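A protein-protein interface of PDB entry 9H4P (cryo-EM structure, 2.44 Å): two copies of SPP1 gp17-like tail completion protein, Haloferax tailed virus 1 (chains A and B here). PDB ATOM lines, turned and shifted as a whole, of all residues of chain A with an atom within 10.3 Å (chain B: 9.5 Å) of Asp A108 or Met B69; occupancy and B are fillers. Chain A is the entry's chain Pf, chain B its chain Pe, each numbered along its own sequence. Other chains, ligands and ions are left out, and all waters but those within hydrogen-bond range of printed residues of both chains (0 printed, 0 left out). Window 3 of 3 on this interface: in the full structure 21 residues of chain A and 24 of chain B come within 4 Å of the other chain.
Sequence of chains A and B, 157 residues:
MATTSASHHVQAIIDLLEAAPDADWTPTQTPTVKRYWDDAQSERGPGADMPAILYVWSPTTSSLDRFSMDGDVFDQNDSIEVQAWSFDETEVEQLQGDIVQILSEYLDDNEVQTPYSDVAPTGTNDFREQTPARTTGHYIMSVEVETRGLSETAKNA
Of the 24 printed residues of chain A, 5 touch a printed residue of chain B. Printed residues of chain A that touch a printed residue of chain B: Ser A104, Glu A105, Leu A107, Asp A108 and Pro A121. Hydrophobic or aromatic side chains of chain A that line the printed part of chain B: Leu A107. Of the 13 printed residues of chain B, 7 touch a printed residue of chain A. Among the printed residues, Asp or Glu carboxylates within 4 Å of a Lys or Arg side-chain nitrogen of the other chain: Asp A108 with Arg B66.
The guanidinium group (NH1) of Arg B66 is in hydrogen-bond range of the backbone carbonyl oxygen (O) of Ser B68 (3.1 Å). NZ of Lys B155 sits at hydrogen-bond distance from O of Asp B70, 2.8 Å away. The backbone carbonyl oxygen (O) of Gly B71 sits at hydrogen-bond distance from the side-chain hydroxyl (OG1) of Thr B153, 2.7 Å away. The backbone carbonyl oxygen (O) of Asp B72 sits at hydrogen-bond distance from the side-chain hydroxyl (OG1) of Thr B153 (3.3 Å). The side-chain amide oxygen (OD1) of Asn B156 is in hydrogen-bond range of the side-chain amino group (NZ) of Lys B155 (3.0 Å).
NH1 of Arg B66 is in salt-bridge range of OD2 of Asp A108, at 2.7 Å. The backbone NH (N) of Ala B154 sits at hydrogen-bond distance from the side-chain hydroxyl (OG) of Ser A104, at 3.0 Å. The backbone NH of Lys B155 sits at hydrogen-bond distance from the backbone carbonyl oxygen of Ser A104, at 3.4 Å.
Among the printed residues, merely in contact across the chains: Asp A108 with Lys B155 (3.4 Å), Leu A107 with Arg B66 (3.5 Å), Leu A107 with Gly B71 (3.5 Å), Asp A108 with Met B69 (3.7 Å), Glu A105 with Ala B154 (3.7 Å), Ser A104 with Thr B153 (3.7 Å), Leu A107 with Thr B153 (3.8 Å), Pro A121 with Phe B74 (3.9 Å), Leu A107 with Lys B155 (3.96 Å) and Leu A107 with Phe B74 (3.97 Å).
No position is printed for both chains.
Of the printed residues of chain B, Leu A107 touches Arg B66, Gly B71, Phe B74, Thr B153 and Lys B155. Of chain B, only Arg B66, Met B69 and Lys B155 come within 4 Å of Asp A108. Printed residues of chain B within 4 Å of Pro A121: Phe B74 (3.9 Å). No residue of chain A comes within 4 Å of Ser B68. Met B69 touches one residue of chain A. No residue of chain A comes within 4 Å of Asp B70. Of the printed residues of chain A, Gly B71 touches Leu A107. Asp B72 touches none of the printed residues of chain A. Printed residues of chain A within 4 Å of Thr B153: Ser A104 (3.7 Å) and Leu A107 (3.8 Å). Of the printed residues of chain A, Ala B154 touches Ser A104 and Glu A105. Printed residues of chain A within 4 Å of Lys B155: Ser A104, Leu A107 and Asp A108. The nearest residue of chain B that does not touch Asp A108 is Gly B71 (4.2 Å). The nearest residue of chain A that does not touch Met B69 is Leu A107 (7.6 Å).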
ATOM      1  N   LEU A  16      20.007  -3.283 -36.603  1.00  0.00           N
ATOM      2  CA  LEU A  16      21.091  -3.091 -35.642  1.00  0.00           C
ATOM      3  C   LEU A  16      21.864  -4.386 -35.388  1.00  0.00           C
ATOM      4  O   LEU A  16      23.092  -4.356 -35.313  1.00  0.00           O
ATOM      5  CB  LEU A  16      20.557  -2.507 -34.329  1.00  0.00           C
ATOM      6  CG  LEU A  16      20.078  -1.055 -34.378  1.00  0.00           C
ATOM      7  CD1 LEU A  16      19.621  -0.593 -33.004  1.00  0.00           C
ATOM      8  CD2 LEU A  16      21.158  -0.125 -34.915  1.00  0.00           C
ATOM      9  N   ILE A 102      25.641  -5.531 -28.028  1.00  0.00           N
ATOM     10  CA  ILE A 102      25.350  -4.890 -29.309  1.00  0.00           C
ATOM     11  C   ILE A 102      24.353  -3.743 -29.114  1.00  0.00           C
ATOM     12  O   ILE A 102      24.640  -2.609 -29.496  1.00  0.00           O
ATOM     13  CB  ILE A 102      24.880  -5.909 -30.377  1.00  0.00           C
ATOM     14  CG1 ILE A 102      25.968  -6.924 -30.756  1.00  0.00           C
ATOM     15  CG2 ILE A 102      24.291  -5.228 -31.612  1.00  0.00           C
ATOM     16  CD1 ILE A 102      27.272  -6.325 -31.257  1.00  0.00           C
ATOM     17  N   LEU A 103      23.201  -4.045 -28.494  1.00  0.00           N
ATOM     18  CA  LEU A 103      22.134  -3.069 -28.310  1.00  0.00           C
ATOM     19  C   LEU A 103      22.401  -2.129 -27.128  1.00  0.00           C
ATOM     20  O   LEU A 103      21.546  -1.298 -26.813  1.00  0.00           O
ATOM     21  CB  LEU A 103      20.779  -3.784 -28.196  1.00  0.00           C
ATOM     22  CG  LEU A 103      20.357  -4.631 -29.403  1.00  0.00           C
ATOM     23  CD1 LEU A 103      19.044  -5.349 -29.139  1.00  0.00           C
ATOM     24  CD2 LEU A 103      20.258  -3.805 -30.680  1.00  0.00           C
ATOM     25  N   SER A 104      23.587  -2.231 -26.502  1.00  0.00           N
ATOM     26  CA  SER A 104      24.031  -1.253 -25.515  1.00  0.00           C
ATOM     27  C   SER A 104      24.879  -0.147 -26.150  1.00  0.00           C
ATOM     28  O   SER A 104      25.172   0.849 -25.489  1.00  0.00           O
ATOM     29  CB  SER A 104      24.725  -1.894 -24.339  1.00  0.00           C
ATOM     30  OG  SER A 104      25.966  -2.457 -24.731  1.00  0.00           O
ATOM     31  N   GLU A 105      25.287  -0.325 -27.418  1.00  0.00           N
ATOM     32  CA  GLU A 105      25.505   0.831 -28.276  1.00  0.00           C
ATOM     33  C   GLU A 105      24.125   1.448 -28.520  1.00  0.00           C
ATOM     34  O   GLU A 105      23.117   0.801 -28.237  1.00  0.00           O
ATOM     35  CB  GLU A 105      26.201   0.439 -29.585  1.00  0.00           C
ATOM     36  CG  GLU A 105      27.647   0.013 -29.411  1.00  0.00           C
ATOM     37  CD  GLU A 105      28.517   0.213 -30.637  1.00  0.00           C
ATOM     38  OE1 GLU A 105      28.651   1.364 -31.080  1.00  0.00           O
ATOM     39  OE2 GLU A 105      29.058  -0.782 -31.143  1.00  0.00           O
ATOM     40  N   TYR A 106      24.068   2.694 -29.015  1.00  0.00           N
ATOM     41  CA  TYR A 106      22.816   3.363 -29.364  1.00  0.00           C
ATOM     42  C   TYR A 106      21.955   3.703 -28.135  1.00  0.00           C
ATOM     43  O   TYR A 106      20.812   4.123 -28.314  1.00  0.00           O
ATOM     44  CB  TYR A 106      22.023   2.589 -30.435  1.00  0.00           C
ATOM     45  CG  TYR A 106      22.834   1.827 -31.458  1.00  0.00           C
ATOM     46  CD1 TYR A 106      23.498   2.490 -32.481  1.00  0.00           C
ATOM     47  CD2 TYR A 106      22.948   0.442 -31.406  1.00  0.00           C
ATOM     48  CE1 TYR A 106      24.255   1.803 -33.420  1.00  0.00           C
ATOM     49  CE2 TYR A 106      23.709  -0.261 -32.331  1.00  0.00           C
ATOM     50  CZ  TYR A 106      24.361   0.423 -33.345  1.00  0.00           C
ATOM     51  OH  TYR A 106      25.100  -0.259 -34.268  1.00  0.00           O
ATOM     52  N   LEU A 107      22.493   3.560 -26.905  1.00  0.00           N
ATOM     53  CA  LEU A 107      21.754   3.740 -25.652  1.00  0.00           C
ATOM     54  C   LEU A 107      21.159   5.145 -25.516  1.00  0.00           C
ATOM     55  O   LEU A 107      20.050   5.286 -25.003  1.00  0.00           O
ATOM     56  CB  LEU A 107      22.648   3.400 -24.450  1.00  0.00           C
ATOM     57  CG  LEU A 107      22.462   2.009 -23.839  1.00  0.00           C
ATOM     58  CD1 LEU A 107      23.568   1.714 -22.837  1.00  0.00           C
ATOM     59  CD2 LEU A 107      21.103   1.865 -23.170  1.00  0.00           C
ATOM     60  N   ASP A 108      21.907   6.169 -25.957  1.00  0.00           N
ATOM     61  CA  ASP A 108      21.440   7.549 -25.999  1.00  0.00           C
ATOM     62  C   ASP A 108      21.767   8.168 -27.358  1.00  0.00           C
ATOM     63  O   ASP A 108      22.240   9.301 -27.441  1.00  0.00           O
ATOM     64  CB  ASP A 108      21.980   8.363 -24.820  1.00  0.00           C
ATOM     65  CG  ASP A 108      21.653   7.742 -23.475  1.00  0.00           C
ATOM     66  OD1 ASP A 108      20.453   7.539 -23.195  1.00  0.00           O
ATOM     67  OD2 ASP A 108      22.603   7.452 -22.727  1.00  0.00           O
ATOM     68  N   ASP A 109      21.510   7.393 -28.415  1.00  0.00           N
ATOM     69  CA  ASP A 109      21.584   7.832 -29.797  1.00  0.00           C
ATOM     70  C   ASP A 109      20.563   8.951 -30.017  1.00  0.00           C
ATOM     71  O   ASP A 109      19.368   8.678 -30.009  1.00  0.00           O
ATOM     72  CB  ASP A 109      21.282   6.625 -30.693  1.00  0.00           C
ATOM     73  CG  ASP A 109      21.189   6.929 -32.175  1.00  0.00           C
ATOM     74  OD1 ASP A 109      21.772   7.932 -32.607  1.00  0.00           O
ATOM     75  OD2 ASP A 109      20.558   6.136 -32.885  1.00  0.00           O
ATOM     76  N   ASN A 110      21.022  10.194 -30.249  1.00  0.00           N
ATOM     77  CA  ASN A 110      20.117  11.310 -30.518  1.00  0.00           C
ATOM     78  C   ASN A 110      19.673  11.320 -31.988  1.00  0.00           C
ATOM     79  O   ASN A 110      19.885  12.312 -32.687  1.00  0.00           O
ATOM     80  CB  ASN A 110      20.682  12.646 -30.022  1.00  0.00           C
ATOM     81  CG  ASN A 110      22.072  12.936 -30.539  1.00  0.00           C
ATOM     82  OD1 ASN A 110      23.056  12.487 -29.964  1.00  0.00           O
ATOM     83  ND2 ASN A 110      22.160  13.685 -31.622  1.00  0.00           N
ATOM     84  N   GLU A 111      19.062  10.210 -32.443  1.00  0.00           N
ATOM     85  CA  GLU A 111      18.611   9.977 -33.814  1.00  0.00           C
ATOM     86  C   GLU A 111      19.751  10.086 -34.841  1.00  0.00           C
ATOM     87  O   GLU A 111      19.506  10.454 -35.990  1.00  0.00           O
ATOM     88  CB  GLU A 111      17.420  10.873 -34.185  1.00  0.00           C
ATOM     89  CG  GLU A 111      16.180  10.686 -33.323  1.00  0.00           C
ATOM     90  CD  GLU A 111      14.991  11.532 -33.744  1.00  0.00           C
ATOM     91  OE1 GLU A 111      14.946  11.950 -34.915  1.00  0.00           O
ATOM     92  OE2 GLU A 111      14.108  11.761 -32.903  1.00  0.00           O
ATOM     93  N   VAL A 112      20.990   9.741 -34.444  1.00  0.00           N
ATOM     94  CA  VAL A 112      22.150   9.762 -35.332  1.00  0.00           C
ATOM     95  C   VAL A 112      22.183   8.462 -36.138  1.00  0.00           C
ATOM     96  O   VAL A 112      22.231   8.506 -37.367  1.00  0.00           O
ATOM     97  CB  VAL A 112      23.478  10.007 -34.577  1.00  0.00           C
ATOM     98  CG1 VAL A 112      24.681  10.031 -35.512  1.00  0.00           C
ATOM     99  CG2 VAL A 112      23.447  11.282 -33.749  1.00  0.00           C
ATOM    100  N   GLN A 113      22.153   7.317 -35.437  1.00  0.00           N
ATOM    101  CA  GLN A 113      22.261   6.005 -36.066  1.00  0.00           C
ATOM    102  C   GLN A 113      20.872   5.487 -36.451  1.00  0.00           C
ATOM    103  O   GLN A 113      20.627   5.161 -37.613  1.00  0.00           O
ATOM    104  CB  GLN A 113      23.056   5.029 -35.183  1.00  0.00           C
ATOM    105  CG  GLN A 113      24.407   5.551 -34.691  1.00  0.00           C
ATOM    106  CD  GLN A 113      25.441   5.856 -35.752  1.00  0.00           C
ATOM    107  OE1 GLN A 113      25.207   5.740 -36.953  1.00  0.00           O
ATOM    108  NE2 GLN A 113      26.621   6.256 -35.307  1.00  0.00           N
ATOM    109  N   THR A 114      19.976   5.450 -35.449  1.00  0.00           N
ATOM    110  CA  THR A 114      18.601   4.967 -35.513  1.00  0.00           C
ATOM    111  C   THR A 114      17.634   6.143 -35.713  1.00  0.00           C
ATOM    112  O   THR A 114      18.062   7.298 -35.666  1.00  0.00           O
ATOM    113  CB  THR A 114      18.237   4.237 -34.206  1.00  0.00           C
ATOM    114  OG1 THR A 114      18.184   5.167 -33.121  1.00  0.00           O
ATOM    115  CG2 THR A 114      19.178   3.107 -33.839  1.00  0.00           C
ATOM    116  N   PRO A 115      16.311   5.906 -35.947  1.00  0.00           N
ATOM    117  CA  PRO A 115      15.300   6.964 -35.827  1.00  0.00           C
ATOM    118  C   PRO A 115      14.770   7.256 -34.413  1.00  0.00           C
ATOM    119  O   PRO A 115      13.705   7.856 -34.277  1.00  0.00           O
ATOM    120  CB  PRO A 115      14.183   6.442 -36.754  1.00  0.00           C
ATOM    121  CG  PRO A 115      14.249   4.937 -36.600  1.00  0.00           C
ATOM    122  CD  PRO A 115      15.725   4.642 -36.439  1.00  0.00           C
ATOM    123  N   TYR A 116      15.522   6.866 -33.364  1.00  0.00           N
ATOM    124  CA  TYR A 116      15.087   6.952 -31.969  1.00  0.00           C
ATOM    125  C   TYR A 116      16.053   7.801 -31.138  1.00  0.00           C
ATOM    126  O   TYR A 116      17.196   7.993 -31.544  1.00  0.00           O
ATOM    127  CB  TYR A 116      14.940   5.550 -31.362  1.00  0.00           C
ATOM    128  CG  TYR A 116      14.018   4.666 -32.160  1.00  0.00           C
ATOM    129  CD1 TYR A 116      12.670   4.982 -32.268  1.00  0.00           C
ATOM    130  CD2 TYR A 116      14.493   3.562 -32.860  1.00  0.00           C
ATOM    131  CE1 TYR A 116      11.809   4.212 -33.029  1.00  0.00           C
ATOM    132  CE2 TYR A 116      13.641   2.774 -33.622  1.00  0.00           C
ATOM    133  CZ  TYR A 116      12.297   3.106 -33.707  1.00  0.00           C
ATOM    134  OH  TYR A 116      11.442   2.350 -34.451  1.00  0.00           O
ATOM    135  N   SER A 117      15.585   8.290 -29.970  1.00  0.00           N
ATOM    136  CA  SER A 117      16.394   8.979 -28.964  1.00  0.00           C
ATOM    137  C   SER A 117      17.151   7.993 -28.072  1.00  0.00           C
ATOM    138  O   SER A 117      18.116   8.376 -27.408  1.00  0.00           O
ATOM    139  CB  SER A 117      15.555   9.884 -28.092  1.00  0.00           C
ATOM    140  OG  SER A 117      14.839  10.832 -28.867  1.00  0.00           O
ATOM    141  N   ASP A 118      16.676   6.738 -28.041  1.00  0.00           N
ATOM    142  CA  ASP A 118      17.043   5.742 -27.045  1.00  0.00           C
ATOM    143  C   ASP A 118      16.614   4.366 -27.554  1.00  0.00           C
ATOM    144  O   ASP A 118      15.437   4.159 -27.844  1.00  0.00           O
ATOM    145  CB  ASP A 118      16.381   6.089 -25.701  1.00  0.00           C
ATOM    146  CG  ASP A 118      16.415   5.037 -24.601  1.00  0.00           C
ATOM    147  OD1 ASP A 118      17.062   3.984 -24.778  1.00  0.00           O
ATOM    148  OD2 ASP A 118      15.789   5.289 -23.558  1.00  0.00           O
ATOM    149  N   VAL A 119      17.582   3.446 -27.684  1.00  0.00           N
ATOM    150  CA  VAL A 119      17.336   2.010 -27.775  1.00  0.00           C
ATOM    151  C   VAL A 119      18.067   1.361 -26.597  1.00  0.00           C
ATOM    152  O   VAL A 119      19.280   1.536 -26.465  1.00  0.00           O
ATOM    153  CB  VAL A 119      17.812   1.411 -29.120  1.00  0.00           C
ATOM    154  CG1 VAL A 119      17.744  -0.113 -29.146  1.00  0.00           C
ATOM    155  CG2 VAL A 119      17.076   1.993 -30.320  1.00  0.00           C
ATOM    156  N   ALA A 120      17.344   0.596 -25.761  1.00  0.00           N
ATOM    157  CA  ALA A 120      17.943  -0.007 -24.575  1.00  0.00           C
ATOM    158  C   ALA A 120      17.443  -1.433 -24.338  1.00  0.00           C
ATOM    159  O   ALA A 120      16.239  -1.681 -24.406  1.00  0.00           O
ATOM    160  CB  ALA A 120      17.672   0.864 -23.368  1.00  0.00           C
ATOM    161  N   PRO A 121      18.342  -2.399 -23.993  1.00  0.00           N
ATOM    162  CA  PRO A 121      17.938  -3.593 -23.243  1.00  0.00           C
ATOM    163  C   PRO A 121      17.437  -3.125 -21.872  1.00  0.00           C
ATOM    164  O   PRO A 121      18.085  -2.297 -21.226  1.00  0.00           O
ATOM    165  CB  PRO A 121      19.226  -4.431 -23.088  1.00  0.00           C
ATOM    166  CG  PRO A 121      20.218  -3.819 -24.064  1.00  0.00           C
ATOM    167  CD  PRO A 121      19.793  -2.375 -24.247  1.00  0.00           C
ATOM    168  N   GLU A 146      13.519  -1.849 -25.052  1.00  0.00           N
ATOM    169  CA  GLU A 146      12.613  -0.717 -25.149  1.00  0.00           C
ATOM    170  C   GLU A 146      13.270   0.377 -25.990  1.00  0.00           C
ATOM    171  O   GLU A 146      14.493   0.403 -26.141  1.00  0.00           O
ATOM    172  CB  GLU A 146      12.167  -0.264 -23.758  1.00  0.00           C
ATOM    173  CG  GLU A 146      11.327  -1.304 -23.041  1.00  0.00           C
ATOM    174  CD  GLU A 146      10.951  -0.946 -21.618  1.00  0.00           C
ATOM    175  OE1 GLU A 146      10.441   0.166 -21.405  1.00  0.00           O
ATOM    176  OE2 GLU A 146      11.166  -1.781 -20.730  1.00  0.00           O
ATOM    177  N   THR A 147      12.441   1.261 -26.552  1.00  0.00           N
ATOM    178  CA  THR A 147      12.866   2.134 -27.635  1.00  0.00           C
ATOM    179  C   THR A 147      11.984   3.379 -27.617  1.00  0.00           C
ATOM    180  O   THR A 147      10.759   3.260 -27.619  1.00  0.00           O
ATOM    181  CB  THR A 147      12.816   1.352 -28.957  1.00  0.00           C
ATOM    182  OG1 THR A 147      13.902   0.424 -29.006  1.00  0.00           O
ATOM    183  CG2 THR A 147      12.875   2.225 -30.186  1.00  0.00           C
ATOM    184  N   ARG A 148      12.610   4.566 -27.606  1.00  0.00           N
ATOM    185  CA  ARG A 148      11.878   5.800 -27.353  1.00  0.00           C
ATOM    186  C   ARG A 148      12.333   6.915 -28.294  1.00  0.00           C
ATOM    187  O   ARG A 148      13.525   7.053 -28.565  1.00  0.00           O
ATOM    188  CB  ARG A 148      12.022   6.203 -25.881  1.00  0.00           C
ATOM    189  CG  ARG A 148      11.002   7.230 -25.415  1.00  0.00           C
ATOM    190  CD  ARG A 148      11.183   7.522 -23.940  1.00  0.00           C
ATOM    191  NE  ARG A 148      10.203   8.474 -23.430  1.00  0.00           N
ATOM    192  CZ  ARG A 148      10.110   8.869 -22.164  1.00  0.00           C
ATOM    193  NH1 ARG A 148       9.180   9.741 -21.813  1.00  0.00           N
ATOM    194  NH2 ARG A 148      10.937   8.400 -21.247  1.00  0.00           N
ATOM    195  N   ARG B  66      18.886   1.772 -16.013  1.00  0.00           N
ATOM    196  CA  ARG B  66      19.892   2.800 -16.254  1.00  0.00           C
ATOM    197  C   ARG B  66      20.457   3.291 -14.919  1.00  0.00           C
ATOM    198  O   ARG B  66      19.691   3.575 -13.998  1.00  0.00           O
ATOM    199  CB  ARG B  66      19.267   3.983 -17.006  1.00  0.00           C
ATOM    200  CG  ARG B  66      18.868   3.691 -18.448  1.00  0.00           C
ATOM    201  CD  ARG B  66      20.025   3.431 -19.404  1.00  0.00           C
ATOM    202  NE  ARG B  66      20.964   4.550 -19.415  1.00  0.00           N
ATOM    203  CZ  ARG B  66      21.115   5.431 -20.401  1.00  0.00           C
ATOM    204  NH1 ARG B  66      21.986   6.417 -20.273  1.00  0.00           N
ATOM    205  NH2 ARG B  66      20.404   5.331 -21.512  1.00  0.00           N
ATOM    206  N   PHE B  67      21.790   3.421 -14.836  1.00  0.00           N
ATOM    207  CA  PHE B  67      22.452   3.911 -13.631  1.00  0.00           C
ATOM    208  C   PHE B  67      22.589   5.439 -13.625  1.00  0.00           C
ATOM    209  O   PHE B  67      22.505   6.051 -12.558  1.00  0.00           O
ATOM    210  CB  PHE B  67      23.794   3.201 -13.418  1.00  0.00           C
ATOM    211  CG  PHE B  67      24.475   3.499 -12.103  1.00  0.00           C
ATOM    212  CD1 PHE B  67      23.946   3.035 -10.902  1.00  0.00           C
ATOM    213  CD2 PHE B  67      25.657   4.231 -12.064  1.00  0.00           C
ATOM    214  CE1 PHE B  67      24.577   3.303  -9.695  1.00  0.00           C
ATOM    215  CE2 PHE B  67      26.289   4.497 -10.855  1.00  0.00           C
ATOM    216  CZ  PHE B  67      25.747   4.034  -9.673  1.00  0.00           C
ATOM    217  N   SER B  68      22.821   6.042 -14.805  1.00  0.00           N
ATOM    218  CA  SER B  68      23.080   7.473 -14.949  1.00  0.00           C
ATOM    219  C   SER B  68      22.925   7.909 -16.408  1.00  0.00           C
ATOM    220  O   SER B  68      22.752   7.067 -17.290  1.00  0.00           O
ATOM    221  CB  SER B  68      24.458   7.828 -14.417  1.00  0.00           C
ATOM    222  OG  SER B  68      25.490   7.256 -15.211  1.00  0.00           O
ATOM    223  N   MET B  69      23.024   9.227 -16.656  1.00  0.00           N
ATOM    224  CA  MET B  69      23.038   9.801 -17.999  1.00  0.00           C
ATOM    225  C   MET B  69      24.241   9.338 -18.837  1.00  0.00           C
ATOM    226  O   MET B  69      24.178   9.429 -20.065  1.00  0.00           O
ATOM    227  CB  MET B  69      23.010  11.336 -17.966  1.00  0.00           C
ATOM    228  CG  MET B  69      21.727  11.930 -17.403  1.00  0.00           C
ATOM    229  SD  MET B  69      21.542  13.706 -17.724  1.00  0.00           S
ATOM    230  CE  MET B  69      20.649  14.217 -16.258  1.00  0.00           C
ATOM    231  N   ASP B  70      25.328   8.854 -18.206  1.00  0.00           N
ATOM    232  CA  ASP B  70      26.531   8.444 -18.926  1.00  0.00           C
ATOM    233  C   ASP B  70      26.259   7.237 -19.830  1.00  0.00           C
ATOM    234  O   ASP B  70      26.888   7.106 -20.879  1.00  0.00           O
ATOM    235  CB  ASP B  70      27.701   8.152 -17.979  1.00  0.00           C
ATOM    236  CG  ASP B  70      28.245   9.348 -17.215  1.00  0.00           C
ATOM    237  OD1 ASP B  70      27.808  10.484 -17.486  1.00  0.00           O
ATOM    238  OD2 ASP B  70      29.112   9.130 -16.350  1.00  0.00           O
ATOM    239  N   GLY B  71      25.332   6.359 -19.408  1.00  0.00           N
ATOM    240  CA  GLY B  71      24.985   5.136 -20.121  1.00  0.00           C
ATOM    241  C   GLY B  71      26.104   4.096 -20.086  1.00  0.00           C
ATOM    242  O   GLY B  71      26.114   3.165 -20.890  1.00  0.00           O
ATOM    243  N   ASP B  72      27.013   4.265 -19.118  1.00  0.00           N
ATOM    244  CA  ASP B  72      28.292   3.578 -19.022  1.00  0.00           C
ATOM    245  C   ASP B  72      28.134   2.199 -18.373  1.00  0.00           C
ATOM    246  O   ASP B  72      29.022   1.351 -18.500  1.00  0.00           O
ATOM    247  CB  ASP B  72      29.250   4.456 -18.210  1.00  0.00           C
ATOM    248  CG  ASP B  72      30.715   4.099 -18.344  1.00  0.00           C
ATOM    249  OD1 ASP B  72      31.208   4.046 -19.484  1.00  0.00           O
ATOM    250  OD2 ASP B  72      31.354   3.883 -17.301  1.00  0.00           O
ATOM    251  N   VAL B  73      26.997   1.996 -17.680  1.00  0.00           N
ATOM    252  CA  VAL B  73      26.717   0.853 -16.816  1.00  0.00           C
ATOM    253  C   VAL B  73      25.198   0.665 -16.701  1.00  0.00           C
ATOM    254  O   VAL B  73      24.449   1.639 -16.785  1.00  0.00           O
ATOM    255  CB  VAL B  73      27.393   1.043 -15.433  1.00  0.00           C
ATOM    256  CG1 VAL B  73      26.516   0.692 -14.236  1.00  0.00           C
ATOM    257  CG2 VAL B  73      28.742   0.341 -15.341  1.00  0.00           C
ATOM    258  N   PHE B  74      24.759  -0.590 -16.494  1.00  0.00           N
ATOM    259  CA  PHE B  74      23.414  -0.913 -16.030  1.00  0.00           C
ATOM    260  C   PHE B  74      23.453  -1.333 -14.558  1.00  0.00           C
ATOM    261  O   PHE B  74      24.355  -2.062 -14.145  1.00  0.00           O
ATOM    262  CB  PHE B  74      22.814  -2.077 -16.829  1.00  0.00           C
ATOM    263  CG  PHE B  74      22.626  -1.878 -18.314  1.00  0.00           C
ATOM    264  CD1 PHE B  74      21.677  -0.987 -18.806  1.00  0.00           C
ATOM    265  CD2 PHE B  74      23.355  -2.634 -19.224  1.00  0.00           C
ATOM    266  CE1 PHE B  74      21.491  -0.832 -20.173  1.00  0.00           C
ATOM    267  CE2 PHE B  74      23.165  -2.483 -20.591  1.00  0.00           C
ATOM    268  CZ  PHE B  74      22.236  -1.578 -21.063  1.00  0.00           C
ATOM    269  N   THR B 153      28.535  -1.628 -20.440  1.00  0.00           N
ATOM    270  CA  THR B 153      27.892  -1.349 -21.724  1.00  0.00           C
ATOM    271  C   THR B 153      28.946  -1.075 -22.803  1.00  0.00           C
ATOM    272  O   THR B 153      30.104  -0.803 -22.488  1.00  0.00           O
ATOM    273  CB  THR B 153      26.929  -0.150 -21.658  1.00  0.00           C
ATOM    274  OG1 THR B 153      27.688   1.055 -21.552  1.00  0.00           O
ATOM    275  CG2 THR B 153      25.919  -0.211 -20.532  1.00  0.00           C
ATOM    276  N   ALA B 154      28.515  -1.104 -24.076  1.00  0.00           N
ATOM    277  CA  ALA B 154      29.366  -0.819 -25.225  1.00  0.00           C
ATOM    278  C   ALA B 154      29.384   0.671 -25.589  1.00  0.00           C
ATOM    279  O   ALA B 154      30.257   1.085 -26.347  1.00  0.00           O
ATOM    280  CB  ALA B 154      28.960  -1.682 -26.398  1.00  0.00           C
ATOM    281  N   LYS B 155      28.448   1.469 -25.045  1.00  0.00           N
ATOM    282  CA  LYS B 155      28.135   2.834 -25.473  1.00  0.00           C
ATOM    283  C   LYS B 155      29.374   3.719 -25.660  1.00  0.00           C
ATOM    284  O   LYS B 155      29.496   4.384 -26.688  1.00  0.00           O
ATOM    285  CB  LYS B 155      27.141   3.482 -24.500  1.00  0.00           C
ATOM    286  CG  LYS B 155      26.715   4.905 -24.840  1.00  0.00           C
ATOM    287  CD  LYS B 155      25.894   5.568 -23.761  1.00  0.00           C
ATOM    288  CE  LYS B 155      25.695   7.048 -24.004  1.00  0.00           C
ATOM    289  NZ  LYS B 155      26.866   7.845 -23.571  1.00  0.00           N
ATOM    290  N   ASN B 156      30.280   3.720 -24.668  1.00  0.00           N
ATOM    291  CA  ASN B 156      31.402   4.648 -24.583  1.00  0.00           C
ATOM    292  C   ASN B 156      32.717   4.037 -25.095  1.00  0.00           C
ATOM    293  O   ASN B 156      33.743   4.715 -25.065  1.00  0.00           O
ATOM    294  CB  ASN B 156      31.525   5.221 -23.164  1.00  0.00           C
ATOM    295  CG  ASN B 156      30.277   5.927 -22.673  1.00  0.00           C
ATOM    296  OD1 ASN B 156      29.624   6.653 -23.418  1.00  0.00           O
ATOM    297  ND2 ASN B 156      29.945   5.731 -21.409  1.00  0.00           N
